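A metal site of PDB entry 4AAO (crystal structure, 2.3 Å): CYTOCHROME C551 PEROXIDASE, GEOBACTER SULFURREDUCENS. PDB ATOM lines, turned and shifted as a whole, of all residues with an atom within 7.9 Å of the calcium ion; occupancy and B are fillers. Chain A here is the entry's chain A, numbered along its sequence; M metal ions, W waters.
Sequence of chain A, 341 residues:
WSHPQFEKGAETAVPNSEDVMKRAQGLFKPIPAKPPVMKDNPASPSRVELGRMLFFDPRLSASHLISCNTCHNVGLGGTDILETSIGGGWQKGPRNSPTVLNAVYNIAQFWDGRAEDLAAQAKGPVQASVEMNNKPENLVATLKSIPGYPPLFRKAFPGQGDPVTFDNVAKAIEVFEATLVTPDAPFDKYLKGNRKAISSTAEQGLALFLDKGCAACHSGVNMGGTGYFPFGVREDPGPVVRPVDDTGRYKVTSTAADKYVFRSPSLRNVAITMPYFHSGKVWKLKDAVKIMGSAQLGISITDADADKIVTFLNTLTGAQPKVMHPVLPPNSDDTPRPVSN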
ATOM      1  N   THR A  79      22.602  23.500   0.032  1.00  0.00           N
ATOM      2  CA  THR A  79      21.630  22.405   0.319  1.00  0.00           C
ATOM      3  C   THR A  79      22.449  21.155   0.644  1.00  0.00           C
ATOM      4  O   THR A  79      23.617  21.308   0.856  1.00  0.00           O
ATOM      5  CB  THR A  79      20.616  22.132  -0.855  1.00  0.00           C
ATOM      6  OG1 THR A  79      19.716  21.072  -0.425  1.00  0.00           O
ATOM      7  CG2 THR A  79      21.355  21.633  -2.147  1.00  0.00           C
ATOM      8  N   ASP A  80      21.904  19.932   0.660  1.00  0.00           N
ATOM      9  CA  ASP A  80      22.759  18.771   1.102  1.00  0.00           C
ATOM     10  C   ASP A  80      22.725  17.587   0.148  1.00  0.00           C
ATOM     11  O   ASP A  80      23.169  16.517   0.527  1.00  0.00           O
ATOM     12  CB  ASP A  80      22.426  18.286   2.519  1.00  0.00           C
ATOM     13  CG  ASP A  80      20.947  18.022   2.720  1.00  0.00           C
ATOM     14  OD1 ASP A  80      20.192  17.981   1.714  1.00  0.00           O
ATOM     15  OD2 ASP A  80      20.495  17.845   3.930  1.00  0.00           O
ATOM     16  N   ILE A  81      22.099  17.761  -1.011  1.00  0.00           N
ATOM     17  CA  ILE A  81      22.017  16.735  -2.053  1.00  0.00           C
ATOM     18  C   ILE A  81      21.463  15.380  -1.546  1.00  0.00           C
ATOM     19  O   ILE A  81      21.888  14.346  -1.947  1.00  0.00           O
ATOM     20  CB  ILE A  81      23.326  16.673  -2.891  1.00  0.00           C
ATOM     21  CG1 ILE A  81      24.429  16.010  -2.050  1.00  0.00           C
ATOM     22  CG2 ILE A  81      23.736  18.121  -3.201  1.00  0.00           C
ATOM     23  CD1 ILE A  81      25.742  15.708  -2.735  1.00  0.00           C
ATOM     24  N   LEU A  82      20.444  15.459  -0.697  1.00  0.00           N
ATOM     25  CA  LEU A  82      19.627  14.358  -0.230  1.00  0.00           C
ATOM     26  C   LEU A  82      18.203  14.722  -0.553  1.00  0.00           C
ATOM     27  O   LEU A  82      17.864  15.939  -0.609  1.00  0.00           O
ATOM     28  CB  LEU A  82      19.698  14.298   1.320  1.00  0.00           C
ATOM     29  CG  LEU A  82      20.953  13.888   2.120  1.00  0.00           C
ATOM     30  CD1 LEU A  82      20.507  12.757   3.077  1.00  0.00           C
ATOM     31  CD2 LEU A  82      22.016  13.340   1.205  1.00  0.00           C
ATOM     32  N   GLU A  83      17.350  13.717  -0.670  1.00  0.00           N
ATOM     33  CA  GLU A  83      15.925  13.968  -0.831  1.00  0.00           C
ATOM     34  C   GLU A  83      15.374  14.775   0.345  1.00  0.00           C
ATOM     35  O   GLU A  83      14.924  15.873   0.149  1.00  0.00           O
ATOM     36  CB  GLU A  83      15.176  12.693  -1.049  1.00  0.00           C
ATOM     37  CG  GLU A  83      15.772  11.876  -2.196  1.00  0.00           C
ATOM     38  CD  GLU A  83      14.889  10.756  -2.633  1.00  0.00           C
ATOM     39  OE1 GLU A  83      13.964  10.420  -1.896  1.00  0.00           O
ATOM     40  OE2 GLU A  83      15.090  10.208  -3.708  1.00  0.00           O
ATOM     41  N   ASN A  96      12.634  18.612   1.353  1.00  0.00           N
ATOM     42  CA  ASN A  96      13.967  18.828   0.778  1.00  0.00           C
ATOM     43  C   ASN A  96      14.529  20.142   1.360  1.00  0.00           C
ATOM     44  O   ASN A  96      13.773  21.110   1.475  1.00  0.00           O
ATOM     45  CB  ASN A  96      13.810  18.939  -0.758  1.00  0.00           C
ATOM     46  CG  ASN A  96      15.168  19.032  -1.474  1.00  0.00           C
ATOM     47  OD1 ASN A  96      15.481  20.071  -2.035  1.00  0.00           O
ATOM     48  ND2 ASN A  96      16.020  17.974  -1.355  1.00  0.00           N
ATOM     49  N   SER A  97      15.795  20.194   1.765  1.00  0.00           N
ATOM     50  CA  SER A  97      16.329  21.462   2.254  1.00  0.00           C
ATOM     51  C   SER A  97      16.577  22.489   1.169  1.00  0.00           C
ATOM     52  O   SER A  97      17.377  22.288   0.301  1.00  0.00           O
ATOM     53  CB  SER A  97      17.559  21.374   3.190  1.00  0.00           C
ATOM     54  OG  SER A  97      18.713  20.927   2.533  1.00  0.00           O
ATOM     55  N   PRO A  98      15.837  23.601   1.205  1.00  0.00           N
ATOM     56  CA  PRO A  98      16.031  24.600   0.199  1.00  0.00           C
ATOM     57  C   PRO A  98      17.376  25.239   0.368  1.00  0.00           C
ATOM     58  O   PRO A  98      17.890  25.206   1.449  1.00  0.00           O
ATOM     59  CB  PRO A  98      14.895  25.617   0.468  1.00  0.00           C
ATOM     60  CG  PRO A  98      14.457  25.425   1.898  1.00  0.00           C
ATOM     61  CD  PRO A  98      15.006  24.058   2.324  1.00  0.00           C
ATOM     62  N   THR A  99      17.958  25.859  -0.677  1.00  0.00           N
ATOM     63  CA  THR A  99      19.275  26.494  -0.498  1.00  0.00           C
ATOM     64  C   THR A  99      19.220  27.695   0.447  1.00  0.00           C
ATOM     65  O   THR A  99      18.243  28.464   0.416  1.00  0.00           O
ATOM     66  CB  THR A  99      19.848  26.945  -1.878  1.00  0.00           C
ATOM     67  OG1 THR A  99      21.152  27.463  -1.708  1.00  0.00           O
ATOM     68  CG2 THR A  99      18.986  28.017  -2.577  1.00  0.00           C
ATOM     69  N   TRP A 111       8.079  25.841   2.192  1.00  0.00           N
ATOM     70  CA  TRP A 111       7.645  24.986   1.073  1.00  0.00           C
ATOM     71  C   TRP A 111       6.151  24.967   0.851  1.00  0.00           C
ATOM     72  O   TRP A 111       5.678  25.013  -0.308  1.00  0.00           O
ATOM     73  CB  TRP A 111       8.115  23.533   1.262  1.00  0.00           C
ATOM     74  CG  TRP A 111       9.461  23.239   0.637  1.00  0.00           C
ATOM     75  CD1 TRP A 111      10.656  22.862   1.270  1.00  0.00           C
ATOM     76  CD2 TRP A 111       9.785  23.278  -0.774  1.00  0.00           C
ATOM     77  NE1 TRP A 111      11.655  22.677   0.363  1.00  0.00           N
ATOM     78  CE2 TRP A 111      11.207  22.911  -0.883  1.00  0.00           C
ATOM     79  CE3 TRP A 111       9.063  23.575  -1.934  1.00  0.00           C
ATOM     80  CZ2 TRP A 111      11.842  22.801  -2.125  1.00  0.00           C
ATOM     81  CZ3 TRP A 111       9.718  23.474  -3.166  1.00  0.00           C
ATOM     82  CH2 TRP A 111      11.079  23.091  -3.266  1.00  0.00           C
ATOM     83  N   ASN A 269      20.646  28.842  -9.074  1.00  0.00           N
ATOM     84  CA  ASN A 269      21.551  27.738  -8.728  1.00  0.00           C
ATOM     85  C   ASN A 269      20.832  26.440  -8.787  1.00  0.00           C
ATOM     86  O   ASN A 269      21.270  25.491  -8.139  1.00  0.00           O
ATOM     87  CB  ASN A 269      22.181  27.934  -7.349  1.00  0.00           C
ATOM     88  CG  ASN A 269      22.988  29.213  -7.260  1.00  0.00           C
ATOM     89  OD1 ASN A 269      24.045  29.368  -7.921  1.00  0.00           O
ATOM     90  ND2 ASN A 269      22.491  30.171  -6.464  1.00  0.00           N
ATOM     91  N   VAL A 270      19.715  26.362  -9.515  1.00  0.00           N
ATOM     92  CA  VAL A 270      18.928  25.135  -9.509  1.00  0.00           C
ATOM     93  C   VAL A 270      19.787  23.976 -10.110  1.00  0.00           C
ATOM     94  O   VAL A 270      19.588  22.807  -9.789  1.00  0.00           O
ATOM     95  CB  VAL A 270      17.598  25.308 -10.248  1.00  0.00           C
ATOM     96  CG1 VAL A 270      17.847  25.635 -11.717  1.00  0.00           C
ATOM     97  CG2 VAL A 270      16.763  24.063 -10.183  1.00  0.00           C
ATOM     98  N   ILE A 272      22.667  23.115  -9.345  1.00  0.00           N
ATOM     99  CA  ILE A 272      23.541  22.453  -8.373  1.00  0.00           C
ATOM    100  C   ILE A 272      22.823  22.178  -7.030  1.00  0.00           C
ATOM    101  O   ILE A 272      23.504  21.921  -5.997  1.00  0.00           O
ATOM    102  CB  ILE A 272      24.860  23.218  -8.124  1.00  0.00           C
ATOM    103  CG1 ILE A 272      24.567  24.574  -7.478  1.00  0.00           C
ATOM    104  CG2 ILE A 272      25.669  23.460  -9.429  1.00  0.00           C
ATOM    105  CD1 ILE A 272      25.790  25.291  -6.961  1.00  0.00           C
ATOM    106  N   THR A 273      21.485  22.248  -7.014  1.00  0.00           N
ATOM    107  CA  THR A 273      20.753  22.028  -5.757  1.00  0.00           C
ATOM    108  C   THR A 273      19.776  20.841  -5.869  1.00  0.00           C
ATOM    109  O   THR A 273      18.762  20.788  -5.150  1.00  0.00           O
ATOM    110  CB  THR A 273      19.962  23.273  -5.310  1.00  0.00           C
ATOM    111  OG1 THR A 273      19.021  23.651  -6.334  1.00  0.00           O
ATOM    112  CG2 THR A 273      20.925  24.446  -5.050  1.00  0.00           C
ATOM    113  N   MET A 274      20.069  19.919  -6.752  1.00  0.00           N
ATOM    114  CA  MET A 274      19.342  18.678  -6.818  1.00  0.00           C
ATOM    115  C   MET A 274      19.364  17.956  -5.499  1.00  0.00           C
ATOM    116  O   MET A 274      20.317  18.131  -4.744  1.00  0.00           O
ATOM    117  CB  MET A 274      19.922  17.768  -7.901  1.00  0.00           C
ATOM    118  CG  MET A 274      21.271  17.122  -7.590  1.00  0.00           C
ATOM    119  SD  MET A 274      22.662  18.242  -7.905  1.00  0.00           S
ATOM    120  CE  MET A 274      22.764  18.102  -9.721  1.00  0.00           C
ATOM    121  N   PRO A 275      18.364  17.109  -5.223  1.00  0.00           N
ATOM    122  CA  PRO A 275      17.198  16.774  -6.051  1.00  0.00           C
ATOM    123  C   PRO A 275      16.079  17.840  -5.918  1.00  0.00           C
ATOM    124  O   PRO A 275      16.229  18.811  -5.152  1.00  0.00           O
ATOM    125  CB  PRO A 275      16.757  15.428  -5.453  1.00  0.00           C
ATOM    126  CG  PRO A 275      17.116  15.511  -4.022  1.00  0.00           C
ATOM    127  CD  PRO A 275      18.433  16.258  -4.005  1.00  0.00           C
ATOM    128  N   TYR A 276      14.972  17.640  -6.616  1.00  0.00           N
ATOM    129  CA  TYR A 276      14.028  18.753  -6.881  1.00  0.00           C
ATOM    130  C   TYR A 276      12.670  18.567  -6.263  1.00  0.00           C
ATOM    131  O   TYR A 276      12.295  17.427  -5.889  1.00  0.00           O
ATOM    132  CB  TYR A 276      13.917  19.056  -8.402  1.00  0.00           C
ATOM    133  CG  TYR A 276      15.288  19.354  -8.971  1.00  0.00           C
ATOM    134  CD1 TYR A 276      15.963  20.536  -8.599  1.00  0.00           C
ATOM    135  CD2 TYR A 276      15.973  18.431  -9.784  1.00  0.00           C
ATOM    136  CE1 TYR A 276      17.236  20.809  -9.000  1.00  0.00           C
ATOM    137  CE2 TYR A 276      17.260  18.758 -10.221  1.00  0.00           C
ATOM    138  CZ  TYR A 276      17.872  19.936  -9.819  1.00  0.00           C
ATOM    139  OH  TYR A 276      19.155  20.289 -10.224  1.00  0.00           O
ATOM    140  N   PHE A 277      11.947  19.713  -6.174  1.00  0.00           N
ATOM    141  CA  PHE A 277      10.551  19.800  -5.636  1.00  0.00           C
ATOM    142  C   PHE A 277      10.473  19.581  -4.148  1.00  0.00           C
ATOM    143  O   PHE A 277      11.444  19.126  -3.562  1.00  0.00           O
ATOM    144  CB  PHE A 277       9.603  18.864  -6.360  1.00  0.00           C
ATOM    145  CG  PHE A 277       9.591  19.063  -7.839  1.00  0.00           C
ATOM    146  CD1 PHE A 277       9.300  20.332  -8.393  1.00  0.00           C
ATOM    147  CD2 PHE A 277       9.816  17.965  -8.706  1.00  0.00           C
ATOM    148  CE1 PHE A 277       9.268  20.512  -9.763  1.00  0.00           C
ATOM    149  CE2 PHE A 277       9.790  18.155 -10.095  1.00  0.00           C
ATOM    150  CZ  PHE A 277       9.511  19.437 -10.608  1.00  0.00           C
ATOM    151  N   HIS A 278       9.333  19.933  -3.529  1.00  0.00           N
ATOM    152  CA  HIS A 278       9.284  19.971  -2.062  1.00  0.00           C
ATOM    153  C   HIS A 278       9.737  18.660  -1.421  1.00  0.00           C
ATOM    154  O   HIS A 278      10.185  18.634  -0.279  1.00  0.00           O
ATOM    155  CB  HIS A 278       7.896  20.319  -1.553  1.00  0.00           C
ATOM    156  CG  HIS A 278       6.891  19.239  -1.797  1.00  0.00           C
ATOM    157  ND1 HIS A 278       6.296  19.042  -3.015  1.00  0.00           N
ATOM    158  CD2 HIS A 278       6.385  18.237  -0.951  1.00  0.00           C
ATOM    159  CE1 HIS A 278       5.439  18.001  -2.935  1.00  0.00           C
ATOM    160  NE2 HIS A 278       5.480  17.508  -1.679  1.00  0.00           N
ATOM    161  N   SER A 279       9.588  17.571  -2.146  1.00  0.00           N
ATOM    162  CA  SER A 279       9.837  16.242  -1.547  1.00  0.00           C
ATOM    163  C   SER A 279      11.262  15.761  -1.845  1.00  0.00           C
ATOM    164  O   SER A 279      11.626  14.697  -1.406  1.00  0.00           O
ATOM    165  CB  SER A 279       8.838  15.248  -2.155  1.00  0.00           C
ATOM    166  OG  SER A 279       9.047  15.238  -3.600  1.00  0.00           O
ATOM    167  N   GLY A 280      12.005  16.492  -2.641  1.00  0.00           N
ATOM    168  CA  GLY A 280      13.263  16.012  -3.250  1.00  0.00           C
ATOM    169  C   GLY A 280      13.199  14.670  -3.976  1.00  0.00           C
ATOM    170  O   GLY A 280      14.214  13.942  -4.042  1.00  0.00           O
ATOM    171  N   VAL A 282      12.514  13.983  -7.258  1.00  0.00           N
ATOM    172  CA  VAL A 282      12.845  14.015  -8.660  1.00  0.00           C
ATOM    173  C   VAL A 282      14.285  14.504  -8.783  1.00  0.00           C
ATOM    174  O   VAL A 282      14.572  15.657  -8.453  1.00  0.00           O
ATOM    175  CB  VAL A 282      11.895  14.958  -9.419  1.00  0.00           C
ATOM    176  CG1 VAL A 282      12.338  15.060 -10.866  1.00  0.00           C
ATOM    177  CG2 VAL A 282      10.488  14.385  -9.353  1.00  0.00           C
HETATM  178 CA    CA M   1      16.743  20.797  -3.976  1.00  0.00          CA
HETATM  179  O   HOH W   1      17.338  22.479  -2.623  1.00  0.00           O
HETATM  180  O   HOH W   2      18.362  19.514  -2.621  1.00  0.00           O
HETATM  181  O   HOH W   3      16.558  22.678  -5.676  1.00  0.00           O
HETATM  182  O   HOH W   4      14.452  21.231  -4.353  1.00  0.00           O
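The backbone carbonyl oxygen (O) of Asn 269 sits close to the side-chain hydroxyl (OG1) of Thr 273 (3.4 Å). The backbone carbonyl oxygen (O) of Asn 96 lies within hydrogen-bond range of the indole nitrogen (NE1) of Trp 111 (2.9 Å). The side-chain amide nitrogen (ND2) of Asn 96 lies within hydrogen-bond range of the backbone carbonyl oxygen (O) of Leu 82, 2.8 Å away. The backbone carbonyl oxygen of Glu 83 is in hydrogen-bond range of the side-chain amide nitrogen of Asn 96 (2.8 Å). The backbone NH of Asn 96 sits at hydrogen-bond distance from the backbone carbonyl oxygen of His 278.
Of the 22 residues printed, 3 come within 4 Å of the calcium ion. Along chain A the residues within 4 Å of the calcium ion span positions 96 to 275. The nearest printed residue that does not touch the calcium ion is Met 274 (4.2 Å).
Water W2 lies within hydrogen-bond range of OG1 of Thr 79 (3.0 Å), ND2 of Asn 96 (3.1 Å) and O of Met 274 (3.2 Å).
Water W1 is bound to the calcium ion, at 2.2 Å. O of Thr 273 binds the calcium ion, at 2.3 Å. Water W4 is bound to the calcium ion (2.4 Å). The calcium ion is bound by the backbone carbonyl oxygen (O) of Pro 275 (2.4 Å). The side-chain amide oxygen (OD1) of Asn 96 is bound to the calcium ion, 2.4 Å away. The calcium ion is bound by water W2 (2.5 Å). The calcium ion is bound by water W3, 2.5 Å away. The calcium ion has seven donor atoms within binding distance.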
